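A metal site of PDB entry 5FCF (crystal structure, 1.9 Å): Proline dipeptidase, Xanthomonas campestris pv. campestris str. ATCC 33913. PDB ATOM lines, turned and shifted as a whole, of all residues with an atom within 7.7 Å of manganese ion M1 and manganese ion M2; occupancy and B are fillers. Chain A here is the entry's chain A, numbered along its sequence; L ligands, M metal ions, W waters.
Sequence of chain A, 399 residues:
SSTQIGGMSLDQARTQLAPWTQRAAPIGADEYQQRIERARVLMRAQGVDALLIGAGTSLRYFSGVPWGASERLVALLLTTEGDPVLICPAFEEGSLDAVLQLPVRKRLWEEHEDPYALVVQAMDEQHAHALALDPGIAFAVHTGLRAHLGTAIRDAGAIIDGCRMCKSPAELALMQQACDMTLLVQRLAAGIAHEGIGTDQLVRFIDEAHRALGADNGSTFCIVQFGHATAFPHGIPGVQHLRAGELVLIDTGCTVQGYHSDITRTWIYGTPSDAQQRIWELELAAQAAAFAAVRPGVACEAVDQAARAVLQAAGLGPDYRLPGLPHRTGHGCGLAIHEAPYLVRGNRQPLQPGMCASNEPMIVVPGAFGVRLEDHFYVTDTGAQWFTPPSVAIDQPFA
O of Thr 264 sits at hydrogen-bond distance from N of Glu 374, 3.1 Å away. The side-chain carboxylate of Glu 374 sits close to a ring nitrogen (NE2) of His 376, 3.0 Å away. The backbone carbonyl oxygen (O) of Asp 262 sits at hydrogen-bond distance from a ring nitrogen (NE2) of His 376, at 2.9 Å. OD2 of Asp 251 sits close to OG1 of Thr 264 (2.9 Å). The side-chain carboxylate (OD2) of Asp 251 lies close to the guanidinium group (NH2) of Arg 372 (2.8 Å). The backbone carbonyl oxygen (O) of Asp 251 lies within hydrogen-bond range of the backbone NH (N) of Ile 223 (2.8 Å). N of Ser 358 lies within hydrogen-bond range of O of His 331 (2.8 Å). The side-chain carboxylate (OE1) of Glu 360 is in salt-bridge range of the guanidinium group (NE) of Arg 372, at 3.9 Å.
Ser 358 touches manganese ion M1. The nearest printed residue that does not touch manganese ion M1 is His 376 (4.1 Å).
OG1 of Thr 264 touches manganese ion M2 (3.7 Å). Four residues have an atom within 4 Å of manganese ion M2: Asp 251, Asp 262, Thr 264 and Glu 374. The nearest printed residue that does not touch manganese ion M2 is Phe 221 (4.1 Å).
Manganese ion M1 is bound by OE2 of Glu 374 (2.1 Å), OD2 of Asp 262 (2.1 Å), O1 of the ligand (2.2 Å), NE2 of His 331 (2.2 Å) and OE2 of Glu 360 (2.2 Å). Manganese ion M1 has five donor atoms within binding distance.
Manganese ion M2 is bound by an oxygen (O1) of the ligand, the side-chain carboxylate (OD1) of Asp 262, the side-chain carboxylate (OD1) of Asp 251, the side-chain carboxylate (OE1) of Glu 374, the side-chain carboxylate (OD2) of Asp 251 and water W1. Manganese ion M2 has six donor atoms within binding distance.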
ATOM      1  N   PHE A 221      24.042   7.168  -8.186  1.00  0.00           N
ATOM      2  CA  PHE A 221      24.238   8.279  -7.199  1.00  0.00           C
ATOM      3  C   PHE A 221      22.813   8.698  -6.793  1.00  0.00           C
ATOM      4  O   PHE A 221      21.855   8.358  -7.523  1.00  0.00           O
ATOM      5  CB  PHE A 221      24.957   9.493  -7.817  1.00  0.00           C
ATOM      6  CG  PHE A 221      24.181  10.086  -8.973  1.00  0.00           C
ATOM      7  CD1 PHE A 221      24.406   9.574 -10.263  1.00  0.00           C
ATOM      8  CD2 PHE A 221      23.275  11.130  -8.799  1.00  0.00           C
ATOM      9  CE1 PHE A 221      23.703  10.054 -11.397  1.00  0.00           C
ATOM     10  CE2 PHE A 221      22.536  11.606  -9.913  1.00  0.00           C
ATOM     11  CZ  PHE A 221      22.761  11.032 -11.201  1.00  0.00           C
ATOM     12  N   ILE A 223      20.964  12.363  -4.980  1.00  0.00           N
ATOM     13  CA  ILE A 223      20.925  13.599  -4.158  1.00  0.00           C
ATOM     14  C   ILE A 223      19.502  13.944  -3.898  1.00  0.00           C
ATOM     15  O   ILE A 223      18.685  13.959  -4.862  1.00  0.00           O
ATOM     16  CB  ILE A 223      21.526  14.737  -4.941  1.00  0.00           C
ATOM     17  CG1 ILE A 223      23.003  14.390  -5.208  1.00  0.00           C
ATOM     18  CG2 ILE A 223      21.414  16.073  -4.123  1.00  0.00           C
ATOM     19  CD1 ILE A 223      23.624  15.481  -6.043  1.00  0.00           C
ATOM     20  N   HIS A 234      25.083  21.192  -5.716  1.00  0.00           N
ATOM     21  CA  HIS A 234      25.377  19.865  -5.201  1.00  0.00           C
ATOM     22  C   HIS A 234      25.219  19.575  -3.740  1.00  0.00           C
ATOM     23  O   HIS A 234      25.617  18.560  -3.359  1.00  0.00           O
ATOM     24  CB  HIS A 234      26.687  19.421  -5.720  1.00  0.00           C
ATOM     25  CG  HIS A 234      26.613  19.096  -7.193  1.00  0.00           C
ATOM     26  ND1 HIS A 234      27.584  19.518  -8.110  1.00  0.00           N
ATOM     27  CD2 HIS A 234      25.619  18.480  -7.926  1.00  0.00           C
ATOM     28  CE1 HIS A 234      27.188  19.170  -9.324  1.00  0.00           C
ATOM     29  NE2 HIS A 234      26.041  18.491  -9.236  1.00  0.00           N
ATOM     30  N   ILE A 250      15.349  15.988  -6.301  1.00  0.00           N
ATOM     31  CA  ILE A 250      15.879  14.655  -6.372  1.00  0.00           C
ATOM     32  C   ILE A 250      16.613  14.520  -7.692  1.00  0.00           C
ATOM     33  O   ILE A 250      16.080  14.748  -8.772  1.00  0.00           O
ATOM     34  CB  ILE A 250      14.781  13.639  -6.361  1.00  0.00           C
ATOM     35  CG1 ILE A 250      13.996  13.693  -5.016  1.00  0.00           C
ATOM     36  CG2 ILE A 250      15.341  12.241  -6.474  1.00  0.00           C
ATOM     37  CD1 ILE A 250      12.835  12.758  -4.884  1.00  0.00           C
ATOM     38  N   ASP A 251      17.892  14.167  -7.572  1.00  0.00           N
ATOM     39  CA  ASP A 251      18.763  14.001  -8.746  1.00  0.00           C
ATOM     40  C   ASP A 251      19.357  12.583  -8.592  1.00  0.00           C
ATOM     41  O   ASP A 251      20.021  12.308  -7.566  1.00  0.00           O
ATOM     42  CB  ASP A 251      19.832  15.118  -8.825  1.00  0.00           C
ATOM     43  CG  ASP A 251      20.721  15.019 -10.063  1.00  0.00           C
ATOM     44  OD1 ASP A 251      20.604  14.064 -10.905  1.00  0.00           O
ATOM     45  OD2 ASP A 251      21.464  15.944 -10.313  1.00  0.00           O
ATOM     46  N   THR A 252      19.090  11.675  -9.538  1.00  0.00           N
ATOM     47  CA  THR A 252      19.526  10.299  -9.370  1.00  0.00           C
ATOM     48  C   THR A 252      19.664   9.654 -10.748  1.00  0.00           C
ATOM     49  O   THR A 252      19.268  10.236 -11.815  1.00  0.00           O
ATOM     50  CB  THR A 252      18.544   9.485  -8.473  1.00  0.00           C
ATOM     51  OG1 THR A 252      19.139   8.202  -8.102  1.00  0.00           O
ATOM     52  CG2 THR A 252      17.139   9.355  -9.075  1.00  0.00           C
ATOM     53  N   GLY A 253      20.127   8.432 -10.742  1.00  0.00           N
ATOM     54  CA  GLY A 253      20.373   7.727 -11.987  1.00  0.00           C
ATOM     55  C   GLY A 253      20.891   6.293 -11.693  1.00  0.00           C
ATOM     56  O   GLY A 253      21.197   5.964 -10.533  1.00  0.00           O
ATOM     57  N   SER A 261      21.753   6.896 -16.897  1.00  0.00           N
ATOM     58  CA  SER A 261      20.773   7.940 -16.680  1.00  0.00           C
ATOM     59  C   SER A 261      21.203   8.963 -15.586  1.00  0.00           C
ATOM     60  O   SER A 261      22.177   8.799 -14.826  1.00  0.00           O
ATOM     61  CB  SER A 261      19.420   7.297 -16.331  1.00  0.00           C
ATOM     62  OG  SER A 261      19.498   6.687 -15.090  1.00  0.00           O
ATOM     63  N   ASP A 262      20.515  10.098 -15.609  1.00  0.00           N
ATOM     64  CA  ASP A 262      20.934  11.254 -14.821  1.00  0.00           C
ATOM     65  C   ASP A 262      19.810  12.312 -14.898  1.00  0.00           C
ATOM     66  O   ASP A 262      19.760  13.038 -15.846  1.00  0.00           O
ATOM     67  CB  ASP A 262      22.343  11.786 -15.304  1.00  0.00           C
ATOM     68  CG  ASP A 262      22.747  13.049 -14.630  1.00  0.00           C
ATOM     69  OD1 ASP A 262      22.199  13.278 -13.498  1.00  0.00           O
ATOM     70  OD2 ASP A 262      23.526  13.897 -15.204  1.00  0.00           O
ATOM     71  N   ILE A 263      18.862  12.212 -13.996  1.00  0.00           N
ATOM     72  CA  ILE A 263      17.626  12.993 -14.070  1.00  0.00           C
ATOM     73  C   ILE A 263      17.341  13.707 -12.771  1.00  0.00           C
ATOM     74  O   ILE A 263      17.492  13.087 -11.670  1.00  0.00           O
ATOM     75  CB  ILE A 263      16.453  12.066 -14.365  1.00  0.00           C
ATOM     76  CG1 ILE A 263      16.574  11.341 -15.714  1.00  0.00           C
ATOM     77  CG2 ILE A 263      15.166  12.881 -14.389  1.00  0.00           C
ATOM     78  CD1 ILE A 263      15.615  10.159 -15.905  1.00  0.00           C
ATOM     79  N   THR A 264      16.928  15.008 -12.892  1.00  0.00           N
ATOM     80  CA  THR A 264      16.605  15.751 -11.723  1.00  0.00           C
ATOM     81  C   THR A 264      15.173  16.150 -11.868  1.00  0.00           C
ATOM     82  O   THR A 264      14.772  16.613 -12.973  1.00  0.00           O
ATOM     83  CB  THR A 264      17.478  17.007 -11.476  1.00  0.00           C
ATOM     84  OG1 THR A 264      18.875  16.649 -11.495  1.00  0.00           O
ATOM     85  CG2 THR A 264      17.116  17.622 -10.149  1.00  0.00           C
ATOM     86  N   ARG A 328      27.168  25.691 -15.941  1.00  0.00           N
ATOM     87  CA  ARG A 328      26.853  25.458 -17.360  1.00  0.00           C
ATOM     88  C   ARG A 328      25.434  24.844 -17.499  1.00  0.00           C
ATOM     89  O   ARG A 328      24.793  24.275 -16.514  1.00  0.00           O
ATOM     90  CB  ARG A 328      27.917  24.491 -17.869  1.00  0.00           C
ATOM     91  CG  ARG A 328      27.707  23.033 -17.372  1.00  0.00           C
ATOM     92  CD  ARG A 328      28.901  22.081 -17.563  1.00  0.00           C
ATOM     93  NE  ARG A 328      28.591  20.837 -16.859  1.00  0.00           N
ATOM     94  CZ  ARG A 328      29.513  20.007 -16.390  1.00  0.00           C
ATOM     95  NH1 ARG A 328      30.787  20.220 -16.621  1.00  0.00           N
ATOM     96  NH2 ARG A 328      29.140  19.016 -15.610  1.00  0.00           N
ATOM     97  N   THR A 329      24.895  24.951 -18.708  1.00  0.00           N
ATOM     98  CA  THR A 329      23.573  24.395 -18.978  1.00  0.00           C
ATOM     99  C   THR A 329      23.470  22.842 -18.987  1.00  0.00           C
ATOM    100  O   THR A 329      22.453  22.240 -18.584  1.00  0.00           O
ATOM    101  CB  THR A 329      23.062  24.997 -20.287  1.00  0.00           C
ATOM    102  OG1 THR A 329      22.697  26.356 -20.003  1.00  0.00           O
ATOM    103  CG2 THR A 329      21.817  24.362 -20.868  1.00  0.00           C
ATOM    104  N   GLY A 330      24.557  22.158 -19.376  1.00  0.00           N
ATOM    105  CA  GLY A 330      24.527  20.727 -19.490  1.00  0.00           C
ATOM    106  C   GLY A 330      25.883  20.127 -19.866  1.00  0.00           C
ATOM    107  O   GLY A 330      26.878  20.880 -20.157  1.00  0.00           O
ATOM    108  N   HIS A 331      25.902  18.793 -19.824  1.00  0.00           N
ATOM    109  CA  HIS A 331      27.034  18.006 -20.079  1.00  0.00           C
ATOM    110  C   HIS A 331      26.699  16.849 -20.944  1.00  0.00           C
ATOM    111  O   HIS A 331      25.671  16.275 -20.830  1.00  0.00           O
ATOM    112  CB  HIS A 331      27.737  17.562 -18.796  1.00  0.00           C
ATOM    113  CG  HIS A 331      26.853  16.750 -17.905  1.00  0.00           C
ATOM    114  ND1 HIS A 331      26.605  15.416 -18.080  1.00  0.00           N
ATOM    115  CD2 HIS A 331      26.018  17.179 -16.916  1.00  0.00           C
ATOM    116  CE1 HIS A 331      25.718  15.019 -17.186  1.00  0.00           C
ATOM    117  NE2 HIS A 331      25.327  16.058 -16.458  1.00  0.00           N
ATOM    118  N   GLY A 332      27.681  16.380 -21.655  1.00  0.00           N
ATOM    119  CA  GLY A 332      27.601  15.042 -22.243  1.00  0.00           C
ATOM    120  C   GLY A 332      27.433  13.910 -21.276  1.00  0.00           C
ATOM    121  O   GLY A 332      27.809  13.960 -20.102  1.00  0.00           O
ATOM    122  N   CYS A 333      26.785  12.837 -21.788  1.00  0.00           N
ATOM    123  CA  CYS A 333      26.516  11.645 -20.989  1.00  0.00           C
ATOM    124  C   CYS A 333      26.668  10.428 -21.855  1.00  0.00           C
ATOM    125  O   CYS A 333      26.362  10.448 -23.072  1.00  0.00           O
ATOM    126  CB  CYS A 333      25.132  11.745 -20.372  1.00  0.00           C
ATOM    127  SG  CYS A 333      24.788  10.542 -19.081  1.00  0.00           S
ATOM    128  N   ILE A 337      28.936   9.587 -16.425  1.00  0.00           N
ATOM    129  CA  ILE A 337      27.938  10.564 -16.144  1.00  0.00           C
ATOM    130  C   ILE A 337      28.226  11.900 -16.847  1.00  0.00           C
ATOM    131  O   ILE A 337      27.282  12.492 -17.450  1.00  0.00           O
ATOM    132  CB  ILE A 337      27.758  10.843 -14.609  1.00  0.00           C
ATOM    133  CG1 ILE A 337      27.393   9.564 -13.878  1.00  0.00           C
ATOM    134  CG2 ILE A 337      26.623  11.875 -14.421  1.00  0.00           C
ATOM    135  CD1 ILE A 337      27.452   9.567 -12.370  1.00  0.00           C
ATOM    136  N   HIS A 338      29.447  12.381 -16.702  1.00  0.00           N
ATOM    137  CA  HIS A 338      29.881  13.603 -17.312  1.00  0.00           C
ATOM    138  C   HIS A 338      30.927  13.220 -18.390  1.00  0.00           C
ATOM    139  O   HIS A 338      31.932  12.634 -18.028  1.00  0.00           O
ATOM    140  CB  HIS A 338      30.490  14.515 -16.271  1.00  0.00           C
ATOM    141  CG  HIS A 338      29.541  14.825 -15.190  1.00  0.00           C
ATOM    142  ND1 HIS A 338      29.567  14.157 -13.962  1.00  0.00           N
ATOM    143  CD2 HIS A 338      28.389  15.546 -15.192  1.00  0.00           C
ATOM    144  CE1 HIS A 338      28.536  14.601 -13.222  1.00  0.00           C
ATOM    145  NE2 HIS A 338      27.894  15.545 -13.912  1.00  0.00           N
ATOM    146  N   ALA A 357      23.367  14.816 -24.346  1.00  0.00           N
ATOM    147  CA  ALA A 357      23.740  15.733 -23.264  1.00  0.00           C
ATOM    148  C   ALA A 357      22.570  16.021 -22.360  1.00  0.00           C
ATOM    149  O   ALA A 357      21.402  15.788 -22.773  1.00  0.00           O
ATOM    150  CB  ALA A 357      24.252  17.039 -23.860  1.00  0.00           C
ATOM    151  N   SER A 358      22.894  16.417 -21.140  1.00  0.00           N
ATOM    152  CA  SER A 358      21.936  16.966 -20.177  1.00  0.00           C
ATOM    153  C   SER A 358      21.489  18.364 -20.495  1.00  0.00           C
ATOM    154  O   SER A 358      22.166  19.157 -21.208  1.00  0.00           O
ATOM    155  CB  SER A 358      22.487  16.937 -18.750  1.00  0.00           C
ATOM    156  OG  SER A 358      23.415  17.965 -18.548  1.00  0.00           O
ATOM    157  N   ASN A 359      20.284  18.671 -20.039  1.00  0.00           N
ATOM    158  CA  ASN A 359      19.726  20.012 -20.231  1.00  0.00           C
ATOM    159  C   ASN A 359      19.108  20.368 -18.844  1.00  0.00           C
ATOM    160  O   ASN A 359      18.031  19.875 -18.434  1.00  0.00           O
ATOM    161  CB  ASN A 359      18.672  20.008 -21.323  1.00  0.00           C
ATOM    162  CG  ASN A 359      18.107  21.412 -21.618  1.00  0.00           C
ATOM    163  OD1 ASN A 359      18.332  22.349 -20.838  1.00  0.00           O
ATOM    164  ND2 ASN A 359      17.266  21.514 -22.648  1.00  0.00           N
ATOM    165  N   GLU A 360      19.857  21.142 -18.068  1.00  0.00           N
ATOM    166  CA  GLU A 360      19.675  21.236 -16.597  1.00  0.00           C
ATOM    167  C   GLU A 360      20.105  22.668 -16.129  1.00  0.00           C
ATOM    168  O   GLU A 360      20.944  22.846 -15.276  1.00  0.00           O
ATOM    169  CB  GLU A 360      20.372  20.117 -15.845  1.00  0.00           C
ATOM    170  CG  GLU A 360      21.807  19.881 -16.258  1.00  0.00           C
ATOM    171  CD  GLU A 360      22.526  18.935 -15.344  1.00  0.00           C
ATOM    172  OE1 GLU A 360      22.343  19.086 -14.113  1.00  0.00           O
ATOM    173  OE2 GLU A 360      23.284  18.087 -15.798  1.00  0.00           O
ATOM    174  N   ARG A 372      16.102  22.801 -10.137  1.00  0.00           N
ATOM    175  CA  ARG A 372      16.850  22.198 -11.223  1.00  0.00           C
ATOM    176  C   ARG A 372      15.884  21.216 -11.881  1.00  0.00           C
ATOM    177  O   ARG A 372      15.379  20.320 -11.201  1.00  0.00           O
ATOM    178  CB  ARG A 372      18.150  21.472 -10.794  1.00  0.00           C
ATOM    179  CG  ARG A 372      18.866  20.827 -12.027  1.00  0.00           C
ATOM    180  CD  ARG A 372      20.271  20.372 -11.742  1.00  0.00           C
ATOM    181  NE  ARG A 372      20.412  19.287 -10.754  1.00  0.00           N
ATOM    182  CZ  ARG A 372      20.899  19.378  -9.492  1.00  0.00           C
ATOM    183  NH1 ARG A 372      21.038  20.576  -8.915  1.00  0.00           N
ATOM    184  NH2 ARG A 372      21.175  18.254  -8.775  1.00  0.00           N
ATOM    185  N   GLU A 374      16.190  18.548 -14.862  1.00  0.00           N
ATOM    186  CA  GLU A 374      17.193  17.805 -15.662  1.00  0.00           C
ATOM    187  C   GLU A 374      16.612  16.639 -16.409  1.00  0.00           C
ATOM    188  O   GLU A 374      16.178  15.650 -15.811  1.00  0.00           O
ATOM    189  CB  GLU A 374      18.403  17.335 -14.789  1.00  0.00           C
ATOM    190  CG  GLU A 374      19.413  16.534 -15.626  1.00  0.00           C
ATOM    191  CD  GLU A 374      20.648  16.027 -14.840  1.00  0.00           C
ATOM    192  OE1 GLU A 374      20.481  15.864 -13.601  1.00  0.00           O
ATOM    193  OE2 GLU A 374      21.653  15.794 -15.563  1.00  0.00           O
ATOM    194  N   ASP A 375      16.660  16.757 -17.732  1.00  0.00           N
ATOM    195  CA  ASP A 375      16.350  15.690 -18.677  1.00  0.00           C
ATOM    196  C   ASP A 375      17.475  15.742 -19.752  1.00  0.00           C
ATOM    197  O   ASP A 375      18.082  16.830 -20.022  1.00  0.00           O
ATOM    198  CB  ASP A 375      15.000  15.928 -19.286  1.00  0.00           C
ATOM    199  CG  ASP A 375      13.873  16.002 -18.242  1.00  0.00           C
ATOM    200  OD1 ASP A 375      13.669  17.070 -17.506  1.00  0.00           O
ATOM    201  OD2 ASP A 375      13.261  14.932 -18.114  1.00  0.00           O
ATOM    202  N   HIS A 376      17.800  14.570 -20.282  1.00  0.00           N
ATOM    203  CA  HIS A 376      18.803  14.477 -21.339  1.00  0.00           C
ATOM    204  C   HIS A 376      18.126  14.348 -22.688  1.00  0.00           C
ATOM    205  O   HIS A 376      16.954  13.893 -22.771  1.00  0.00           O
ATOM    206  CB  HIS A 376      19.675  13.258 -21.072  1.00  0.00           C
ATOM    207  CG  HIS A 376      20.560  13.435 -19.873  1.00  0.00           C
ATOM    208  ND1 HIS A 376      21.847  12.932 -19.815  1.00  0.00           N
ATOM    209  CD2 HIS A 376      20.358  14.090 -18.709  1.00  0.00           C
ATOM    210  CE1 HIS A 376      22.386  13.221 -18.669  1.00  0.00           C
ATOM    211  NE2 HIS A 376      21.515  13.933 -17.965  1.00  0.00           N
HETATM  212  P1  LIG L   1      24.603  17.055 -12.495  1.00  0.00           P
HETATM  213  O1  LIG L   1      23.390  16.018 -12.906  1.00  0.00           O
HETATM  214  O2  LIG L   1      24.976  16.725 -11.079  1.00  0.00           O
HETATM  215  O3  LIG L   1      25.906  17.287 -13.239  1.00  0.00           O
HETATM  216  O4  LIG L   1      24.014  18.462 -12.386  1.00  0.00           O
HETATM  217 MN    MN M   1      23.633  16.010 -15.065  1.00  0.00          MN
HETATM  218 MN    MN M   2      22.031  14.964 -12.267  1.00  0.00          MN
HETATM  219  O   HOH W   1      23.933  14.325 -10.921  1.00  0.00           O
